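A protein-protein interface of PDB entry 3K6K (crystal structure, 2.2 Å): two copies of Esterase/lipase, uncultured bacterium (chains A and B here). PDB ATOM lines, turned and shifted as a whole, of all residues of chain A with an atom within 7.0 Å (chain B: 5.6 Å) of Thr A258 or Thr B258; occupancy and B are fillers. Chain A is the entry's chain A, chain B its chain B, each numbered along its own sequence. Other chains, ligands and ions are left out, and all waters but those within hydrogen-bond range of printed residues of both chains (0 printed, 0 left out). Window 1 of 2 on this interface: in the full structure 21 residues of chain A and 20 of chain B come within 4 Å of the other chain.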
ATOM      1  N   SER A 196     -11.225  20.177   9.268  1.00  0.00           N
ATOM      2  CA  SER A 196     -12.154  21.071   8.560  1.00  0.00           C
ATOM      3  C   SER A 196     -13.580  20.874   9.081  1.00  0.00           C
ATOM      4  O   SER A 196     -14.382  21.815   9.052  1.00  0.00           O
ATOM      5  CB  SER A 196     -12.104  20.898   7.016  1.00  0.00           C
ATOM      6  OG  SER A 196     -12.326  19.545   6.611  1.00  0.00           O
ATOM      7  N   VAL A 233     -10.881   6.511   3.724  1.00  0.00           N
ATOM      8  CA  VAL A 233      -9.795   7.050   4.503  1.00  0.00           C
ATOM      9  C   VAL A 233      -9.133   5.986   5.450  1.00  0.00           C
ATOM     10  O   VAL A 233      -7.926   6.009   5.686  1.00  0.00           O
ATOM     11  CB  VAL A 233     -10.267   8.353   5.180  1.00  0.00           C
ATOM     12  CG1 VAL A 233      -9.619   8.577   6.443  1.00  0.00           C
ATOM     13  CG2 VAL A 233     -10.027   9.540   4.248  1.00  0.00           C
ATOM     14  N   ILE A 245      -7.783  14.710  -7.209  1.00  0.00           N
ATOM     15  CA  ILE A 245      -8.794  15.261  -6.301  1.00  0.00           C
ATOM     16  C   ILE A 245      -8.913  16.804  -6.514  1.00  0.00           C
ATOM     17  O   ILE A 245      -7.913  17.546  -6.550  1.00  0.00           O
ATOM     18  CB  ILE A 245      -8.467  14.923  -4.791  1.00  0.00           C
ATOM     19  CG1 ILE A 245      -8.226  13.431  -4.589  1.00  0.00           C
ATOM     20  CG2 ILE A 245      -9.623  15.343  -3.869  1.00  0.00           C
ATOM     21  CD1 ILE A 245      -7.581  13.138  -3.366  1.00  0.00           C
ATOM     22  N   VAL A 247     -11.071  20.250  -4.858  1.00  0.00           N
ATOM     23  CA  VAL A 247     -11.946  20.595  -3.738  1.00  0.00           C
ATOM     24  C   VAL A 247     -11.861  22.110  -3.530  1.00  0.00           C
ATOM     25  O   VAL A 247     -10.919  22.760  -4.034  1.00  0.00           O
ATOM     26  CB  VAL A 247     -11.504  19.760  -2.452  1.00  0.00           C
ATOM     27  CG1 VAL A 247     -10.019  20.091  -2.033  1.00  0.00           C
ATOM     28  CG2 VAL A 247     -12.468  19.889  -1.289  1.00  0.00           C
ATOM     29  N   LEU A 253     -15.632  19.294   4.580  1.00  0.00           N
ATOM     30  CA  LEU A 253     -15.007  18.020   4.156  1.00  0.00           C
ATOM     31  C   LEU A 253     -13.647  18.233   3.396  1.00  0.00           C
ATOM     32  O   LEU A 253     -13.172  17.388   2.630  1.00  0.00           O
ATOM     33  CB  LEU A 253     -15.981  17.191   3.309  1.00  0.00           C
ATOM     34  CG  LEU A 253     -17.392  16.896   3.853  1.00  0.00           C
ATOM     35  CD1 LEU A 253     -18.156  15.908   2.976  1.00  0.00           C
ATOM     36  CD2 LEU A 253     -17.275  16.336   5.282  1.00  0.00           C
ATOM     37  N   LEU A 254     -13.054  19.384   3.608  1.00  0.00           N
ATOM     38  CA  LEU A 254     -11.716  19.648   3.116  1.00  0.00           C
ATOM     39  C   LEU A 254     -10.722  18.653   3.665  1.00  0.00           C
ATOM     40  O   LEU A 254      -9.807  18.253   2.932  1.00  0.00           O
ATOM     41  CB  LEU A 254     -11.228  21.052   3.484  1.00  0.00           C
ATOM     42  CG  LEU A 254      -9.795  21.407   3.011  1.00  0.00           C
ATOM     43  CD1 LEU A 254      -9.715  21.462   1.525  1.00  0.00           C
ATOM     44  CD2 LEU A 254      -9.327  22.784   3.608  1.00  0.00           C
ATOM     45  N   SER A 255     -10.848  18.277   4.940  1.00  0.00           N
ATOM     46  CA  SER A 255      -9.835  17.372   5.488  1.00  0.00           C
ATOM     47  C   SER A 255     -10.053  15.955   4.917  1.00  0.00           C
ATOM     48  O   SER A 255      -9.167  15.131   5.047  1.00  0.00           O
ATOM     49  CB  SER A 255      -9.787  17.385   7.020  1.00  0.00           C
ATOM     50  OG  SER A 255      -9.520  18.691   7.528  1.00  0.00           O
ATOM     51  N   ASP A 256     -11.204  15.689   4.267  1.00  0.00           N
ATOM     52  CA  ASP A 256     -11.407  14.411   3.543  1.00  0.00           C
ATOM     53  C   ASP A 256     -10.436  14.298   2.333  1.00  0.00           C
ATOM     54  O   ASP A 256      -9.796  13.244   2.091  1.00  0.00           O
ATOM     55  CB  ASP A 256     -12.858  14.221   3.030  1.00  0.00           C
ATOM     56  CG  ASP A 256     -13.848  13.654   4.114  1.00  0.00           C
ATOM     57  OD1 ASP A 256     -14.766  12.933   3.733  1.00  0.00           O
ATOM     58  OD2 ASP A 256     -13.729  13.889   5.328  1.00  0.00           O
ATOM     59  N   SER A 257     -10.371  15.382   1.581  1.00  0.00           N
ATOM     60  CA  SER A 257      -9.446  15.510   0.483  1.00  0.00           C
ATOM     61  C   SER A 257      -7.995  15.458   0.903  1.00  0.00           C
ATOM     62  O   SER A 257      -7.248  14.667   0.342  1.00  0.00           O
ATOM     63  CB  SER A 257      -9.740  16.763  -0.341  1.00  0.00           C
ATOM     64  OG  SER A 257     -10.918  16.559  -1.095  1.00  0.00           O
ATOM     65  N   THR A 258      -7.578  16.279   1.856  1.00  0.00           N
ATOM     66  CA  THR A 258      -6.200  16.293   2.275  1.00  0.00           C
ATOM     67  C   THR A 258      -5.870  14.950   2.942  1.00  0.00           C
ATOM     68  O   THR A 258      -4.748  14.397   2.783  1.00  0.00           O
ATOM     69  CB  THR A 258      -5.900  17.442   3.283  1.00  0.00           C
ATOM     70  OG1 THR A 258      -6.679  17.211   4.449  1.00  0.00           O
ATOM     71  CG2 THR A 258      -6.333  18.653   2.817  1.00  0.00           C
ATOM     72  N   THR A 259      -6.816  14.401   3.700  1.00  0.00           N
ATOM     73  CA  THR A 259      -6.539  13.115   4.393  1.00  0.00           C
ATOM     74  C   THR A 259      -6.466  11.904   3.504  1.00  0.00           C
ATOM     75  O   THR A 259      -5.560  11.061   3.662  1.00  0.00           O
ATOM     76  CB  THR A 259      -7.477  12.811   5.551  1.00  0.00           C
ATOM     77  OG1 THR A 259      -7.419  13.885   6.473  1.00  0.00           O
ATOM     78  CG2 THR A 259      -6.996  11.524   6.330  1.00  0.00           C
ATOM     79  N   LEU A 260      -7.404  11.787   2.588  1.00  0.00           N
ATOM     80  CA  LEU A 260      -7.246  10.793   1.550  1.00  0.00           C
ATOM     81  C   LEU A 260      -5.935  10.942   0.769  1.00  0.00           C
ATOM     82  O   LEU A 260      -5.351   9.944   0.287  1.00  0.00           O
ATOM     83  CB  LEU A 260      -8.383  10.906   0.561  1.00  0.00           C
ATOM     84  CG  LEU A 260      -8.979   9.743  -0.270  1.00  0.00           C
ATOM     85  CD1 LEU A 260      -9.110  10.144  -1.763  1.00  0.00           C
ATOM     86  CD2 LEU A 260      -8.465   8.300  -0.032  1.00  0.00           C
ATOM     87  N   ALA A 261      -5.505  12.171   0.555  1.00  0.00           N
ATOM     88  CA  ALA A 261      -4.231  12.377  -0.151  1.00  0.00           C
ATOM     89  C   ALA A 261      -3.102  11.847   0.766  1.00  0.00           C
ATOM     90  O   ALA A 261      -2.239  11.106   0.320  1.00  0.00           O
ATOM     91  CB  ALA A 261      -4.034  13.873  -0.525  1.00  0.00           C
ATOM     92  N   GLU A 262      -3.123  12.220   2.050  1.00  0.00           N
ATOM     93  CA  GLU A 262      -2.127  11.712   2.965  1.00  0.00           C
ATOM     94  C   GLU A 262      -1.972  10.183   2.816  1.00  0.00           C
ATOM     95  O   GLU A 262      -0.860   9.659   2.482  1.00  0.00           O
ATOM     96  CB  GLU A 262      -2.492  12.062   4.413  1.00  0.00           C
ATOM     97  CG  GLU A 262      -1.397  11.780   5.412  1.00  0.00           C
ATOM     98  CD  GLU A 262      -1.746  12.338   6.724  1.00  0.00           C
ATOM     99  OE1 GLU A 262      -1.302  13.428   7.057  1.00  0.00           O
ATOM    100  OE2 GLU A 262      -2.564  11.730   7.414  1.00  0.00           O
ATOM    101  N   ARG A 263      -3.094   9.486   2.969  1.00  0.00           N
ATOM    102  CA  ARG A 263      -3.100   8.070   3.136  1.00  0.00           C
ATOM    103  C   ARG A 263      -2.971   7.379   1.790  1.00  0.00           C
ATOM    104  O   ARG A 263      -2.291   6.331   1.628  1.00  0.00           O
ATOM    105  CB  ARG A 263      -4.359   7.598   3.896  1.00  0.00           C
ATOM    106  CG  ARG A 263      -4.601   8.346   5.267  1.00  0.00           C
ATOM    107  CD  ARG A 263      -3.344   8.302   6.209  1.00  0.00           C
ATOM    108  NE  ARG A 263      -3.604   9.013   7.476  1.00  0.00           N
ATOM    109  CZ  ARG A 263      -4.300   8.511   8.504  1.00  0.00           C
ATOM    110  NH1 ARG A 263      -4.784   7.273   8.431  1.00  0.00           N
ATOM    111  NH2 ARG A 263      -4.519   9.243   9.603  1.00  0.00           N
ATOM    112  N   ALA A 264      -3.599   7.934   0.789  1.00  0.00           N
ATOM    113  CA  ALA A 264      -3.414   7.280  -0.500  1.00  0.00           C
ATOM    114  C   ALA A 264      -1.896   7.411  -0.919  1.00  0.00           C
ATOM    115  O   ALA A 264      -1.279   6.440  -1.391  1.00  0.00           O
ATOM    116  CB  ALA A 264      -4.353   7.792  -1.486  1.00  0.00           C
ATOM    117  N   LEU A 273      -3.728  16.848  -5.906  1.00  0.00           N
ATOM    118  CA  LEU A 273      -4.814  17.468  -5.236  1.00  0.00           C
ATOM    119  C   LEU A 273      -4.680  18.954  -5.481  1.00  0.00           C
ATOM    120  O   LEU A 273      -3.601  19.500  -5.217  1.00  0.00           O
ATOM    121  CB  LEU A 273      -4.661  17.192  -3.781  1.00  0.00           C
ATOM    122  CG  LEU A 273      -5.603  17.622  -2.642  1.00  0.00           C
ATOM    123  CD1 LEU A 273      -4.885  18.515  -1.677  1.00  0.00           C
ATOM    124  CD2 LEU A 273      -6.957  18.162  -3.063  1.00  0.00           C
ATOM    125  N   ILE A 275      -6.711  22.588  -4.391  1.00  0.00           N
ATOM    126  CA  ILE A 275      -7.706  23.199  -3.551  1.00  0.00           C
ATOM    127  C   ILE A 275      -8.023  24.579  -4.069  1.00  0.00           C
ATOM    128  O   ILE A 275      -7.089  25.385  -4.249  1.00  0.00           O
ATOM    129  CB  ILE A 275      -7.181  23.330  -2.147  1.00  0.00           C
ATOM    130  CG1 ILE A 275      -6.874  21.930  -1.573  1.00  0.00           C
ATOM    131  CG2 ILE A 275      -8.221  24.034  -1.315  1.00  0.00           C
ATOM    132  CD1 ILE A 275      -6.150  22.022  -0.233  1.00  0.00           C
ATOM    133  N   LEU B 254       5.615  13.765   5.250  1.00  0.00           N
ATOM    134  CA  LEU B 254       4.547  13.773   4.220  1.00  0.00           C
ATOM    135  C   LEU B 254       3.442  14.623   4.795  1.00  0.00           C
ATOM    136  O   LEU B 254       2.922  15.460   4.111  1.00  0.00           O
ATOM    137  CB  LEU B 254       3.988  12.380   3.908  1.00  0.00           C
ATOM    138  CG  LEU B 254       2.792  12.330   2.925  1.00  0.00           C
ATOM    139  CD1 LEU B 254       3.130  12.799   1.500  1.00  0.00           C
ATOM    140  CD2 LEU B 254       2.258  10.891   2.846  1.00  0.00           C
ATOM    141  N   SER B 255       3.126  14.415   6.084  1.00  0.00           N
ATOM    142  CA  SER B 255       2.043  15.199   6.708  1.00  0.00           C
ATOM    143  C   SER B 255       2.371  16.662   6.837  1.00  0.00           C
ATOM    144  O   SER B 255       1.450  17.445   7.044  1.00  0.00           O
ATOM    145  CB  SER B 255       1.543  14.669   8.059  1.00  0.00           C
ATOM    146  OG  SER B 255       1.330  13.280   8.046  1.00  0.00           O
ATOM    147  N   ASP B 256       3.624  17.065   6.639  1.00  0.00           N
ATOM    148  CA  ASP B 256       3.876  18.505   6.664  1.00  0.00           C
ATOM    149  C   ASP B 256       3.217  19.145   5.420  1.00  0.00           C
ATOM    150  O   ASP B 256       2.692  20.290   5.481  1.00  0.00           O
ATOM    151  CB  ASP B 256       5.356  18.847   6.739  1.00  0.00           C
ATOM    152  CG  ASP B 256       5.940  18.885   8.182  1.00  0.00           C
ATOM    153  OD1 ASP B 256       6.915  19.656   8.375  1.00  0.00           O
ATOM    154  OD2 ASP B 256       5.495  18.138   9.121  1.00  0.00           O
ATOM    155  N   SER B 257       3.256  18.402   4.311  1.00  0.00           N
ATOM    156  CA  SER B 257       2.761  18.885   3.029  1.00  0.00           C
ATOM    157  C   SER B 257       1.253  18.752   2.966  1.00  0.00           C
ATOM    158  O   SER B 257       0.612  19.602   2.374  1.00  0.00           O
ATOM    159  CB  SER B 257       3.386  18.119   1.840  1.00  0.00           C
ATOM    160  OG  SER B 257       4.804  18.328   1.780  1.00  0.00           O
ATOM    161  N   THR B 258       0.683  17.677   3.506  1.00  0.00           N
ATOM    162  CA  THR B 258      -0.733  17.592   3.436  1.00  0.00           C
ATOM    163  C   THR B 258      -1.403  18.559   4.404  1.00  0.00           C
ATOM    164  O   THR B 258      -2.417  19.213   4.028  1.00  0.00           O
ATOM    165  CB  THR B 258      -1.255  16.188   3.548  1.00  0.00           C
ATOM    166  OG1 THR B 258      -0.814  15.595   4.770  1.00  0.00           O
ATOM    167  CG2 THR B 258      -0.825  15.312   2.282  1.00  0.00           C
ATOM    168  N   THR B 259      -0.818  18.720   5.610  1.00  0.00           N
ATOM    169  CA  THR B 259      -1.148  19.832   6.521  1.00  0.00           C
ATOM    170  C   THR B 259      -0.953  21.269   5.962  1.00  0.00           C
ATOM    171  O   THR B 259      -1.855  22.095   6.087  1.00  0.00           O
ATOM    172  CB  THR B 259      -0.399  19.691   7.912  1.00  0.00           C
ATOM    173  OG1 THR B 259      -0.612  18.374   8.461  1.00  0.00           O
ATOM    174  CG2 THR B 259      -0.946  20.707   8.900  1.00  0.00           C
ATOM    175  N   LEU B 260       0.219  21.604   5.400  1.00  0.00           N
ATOM    176  CA  LEU B 260       0.392  22.918   4.778  1.00  0.00           C
ATOM    177  C   LEU B 260      -0.786  23.102   3.799  1.00  0.00           C
ATOM    178  O   LEU B 260      -1.504  24.084   3.903  1.00  0.00           O
ATOM    179  CB  LEU B 260       1.695  23.040   3.974  1.00  0.00           C
ATOM    180  CG  LEU B 260       2.517  24.337   4.094  1.00  0.00           C
ATOM    181  CD1 LEU B 260       3.207  24.838   2.872  1.00  0.00           C
ATOM    182  CD2 LEU B 260       1.746  25.483   4.759  1.00  0.00           C
ATOM    183  N   ALA B 261      -0.980  22.172   2.859  1.00  0.00           N
ATOM    184  CA  ALA B 261      -2.072  22.289   1.870  1.00  0.00           C
ATOM    185  C   ALA B 261      -3.427  22.473   2.538  1.00  0.00           C
ATOM    186  O   ALA B 261      -4.169  23.332   2.144  1.00  0.00           O
ATOM    187  CB  ALA B 261      -2.113  21.098   0.881  1.00  0.00           C
ATOM    188  N   GLU B 262      -3.716  21.689   3.577  1.00  0.00           N
ATOM    189  CA  GLU B 262      -4.934  21.852   4.351  1.00  0.00           C
ATOM    190  C   GLU B 262      -5.142  23.246   4.997  1.00  0.00           C
ATOM    191  O   GLU B 262      -6.286  23.822   4.926  1.00  0.00           O
ATOM    192  CB  GLU B 262      -5.006  20.826   5.464  1.00  0.00           C
ATOM    193  CG  GLU B 262      -6.374  20.805   6.134  1.00  0.00           C
ATOM    194  CD  GLU B 262      -6.279  20.246   7.546  1.00  0.00           C
ATOM    195  OE1 GLU B 262      -7.097  19.412   7.942  1.00  0.00           O
ATOM    196  OE2 GLU B 262      -5.333  20.593   8.265  1.00  0.00           O
ATOM    197  N   ARG B 263      -4.075  23.783   5.620  1.00  0.00           N
ATOM    198  CA  ARG B 263      -4.217  25.022   6.338  1.00  0.00           C
ATOM    199  C   ARG B 263      -4.158  26.193   5.397  1.00  0.00           C
ATOM    200  O   ARG B 263      -4.874  27.199   5.570  1.00  0.00           O
ATOM    201  CB  ARG B 263      -3.243  25.177   7.539  1.00  0.00           C
ATOM    202  CG  ARG B 263      -3.352  24.068   8.616  1.00  0.00           C
ATOM    203  CD  ARG B 263      -4.835  23.649   8.950  1.00  0.00           C
ATOM    204  NE  ARG B 263      -4.784  22.496   9.861  1.00  0.00           N
ATOM    205  CZ  ARG B 263      -4.398  22.573  11.142  1.00  0.00           C
ATOM    206  NH1 ARG B 263      -4.091  23.750  11.669  1.00  0.00           N
ATOM    207  NH2 ARG B 263      -4.309  21.482  11.907  1.00  0.00           N
ATOM    208  N   LEU B 273      -0.864  20.119  -4.825  1.00  0.00           N
ATOM    209  CA  LEU B 273      -0.009  19.158  -4.135  1.00  0.00           C
ATOM    210  C   LEU B 273       0.064  17.932  -5.051  1.00  0.00           C
ATOM    211  O   LEU B 273      -0.943  17.502  -5.638  1.00  0.00           O
ATOM    212  CB  LEU B 273      -0.674  18.598  -2.887  1.00  0.00           C
ATOM    213  CG  LEU B 273      -0.045  18.172  -1.540  1.00  0.00           C
ATOM    214  CD1 LEU B 273      -0.989  17.157  -0.684  1.00  0.00           C
ATOM    215  CD2 LEU B 273       1.471  17.796  -1.490  1.00  0.00           C
ATOM    216  N   ILE B 275       1.782  14.033  -4.690  1.00  0.00           N
ATOM    217  CA  ILE B 275       2.494  12.979  -4.000  1.00  0.00           C
ATOM    218  C   ILE B 275       2.979  11.850  -4.950  1.00  0.00           C
ATOM    219  O   ILE B 275       2.181  11.206  -5.624  1.00  0.00           O
ATOM    220  CB  ILE B 275       1.578  12.391  -2.981  1.00  0.00           C
ATOM    221  CG1 ILE B 275       0.870  13.549  -2.241  1.00  0.00           C
ATOM    222  CG2 ILE B 275       2.339  11.381  -2.066  1.00  0.00           C
ATOM    223  CD1 ILE B 275      -0.105  13.005  -1.164  1.00  0.00           C
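The side-chain carboxylate of Glu B262 sits at hydrogen-bond distance from the side-chain hydroxyl of Ser A255.
The backbone NH of Leu B273 sits at hydrogen-bond distance from the backbone carbonyl oxygen of Leu A273.
The side-chain carboxylate (OE1) of Glu A262 sits at hydrogen-bond distance from the side-chain hydroxyl (OG1) of Thr B258.
OE1 of Glu A262 sits at hydrogen-bond distance from OG of Ser B255.
The side-chain carboxylate (OE2) of Glu B262 lies within salt-bridge range of the guanidinium group (NE) of Arg B263 (2.5 Å).
The backbone carbonyl oxygen (O) of Ser B255 is in hydrogen-bond range of the side-chain hydroxyl (OG1) of Thr B259.
The side-chain carboxylate of Glu A262 is in salt-bridge range of the guanidinium group of Arg A263 (2.9 Å).
O of Ser A255 sits at hydrogen-bond distance from OG1 of Thr A259.
The side-chain hydroxyl (OG) of Ser A196 sits at hydrogen-bond distance from the backbone NH (N) of Ser A255, at 2.6 Å.
N of Leu A254 sits at hydrogen-bond distance from OG of Ser A196, 3.1 Å away.
Leu A254 touches Glu B262.
Thr B258 touches Thr A258.
CG2 of Thr A258 touches CB of Glu B262 (3.7 Å).
Ile B275 touches Ala A261 (CD1 to O, 3.2 Å).
CD2 of Leu B254 touches O of Glu A262 (3.4 Å).
Ala B261 touches Ile A275.
Thr A258 touches just these residues of chain B: Thr B258 and Glu B262.
Of the printed residues of chain B, Ala A261 touches Ile B275.
Printed residues of chain B within 4 Å of Leu A273: Leu B273 (2.8 Å).
Of the printed residues of chain B, Ile A275 touches Ala B261.
Asp B256 touches none of the printed residues of chain A.
Of chain A, only Thr A258 (3.98 Å) and Glu A262 (3.2 Å) come within 4 Å of Thr B258.
Of the printed residues of chain A, Ala B261 touches Ile A275.
Of the printed residues of chain A, Leu B273 touches Leu A273.
The nearest residue of chain B that does not touch Thr A258 is Ala B261 (4.8 Å).
The nearest printed residue of chain B that does not touch Ala A261 is Thr B258 (4.4 Å).
Hydrophobic or aromatic side chains of chain A that line the printed part of chain B: Leu A254 and Ile A275.
Along chain A the printed residues that touch a printed residue of chain B span positions 254 to 275.
Of the 12 printed residues of chain B, 7 touch a printed residue of chain A.
Printed residues of chain B that touch a printed residue of chain A: Leu B254, Ser B255, Thr B258, Ala B261, Glu B262, Leu B273 and Ile B275.
Hydrophobic or aromatic side chains of chain B within 4 Å of the printed part of chain A: Leu B254, Leu B273 and Ile B275.
Leu A254 touches Glu B262, and with the chains exchanged Glu A262 touches Leu B254.
Ser A255 touches Glu B262, and with the chains exchanged Glu A262 touches Ser B255.
Thr B258 touches its own counterpart, Thr A258.
Thr A258 touches Glu B262, and with the chains exchanged Glu A262 touches Thr B258.
Of the 10 pairs that touch across the chains among the printed residues, 10 have their exchanged pair printed and touching as well.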
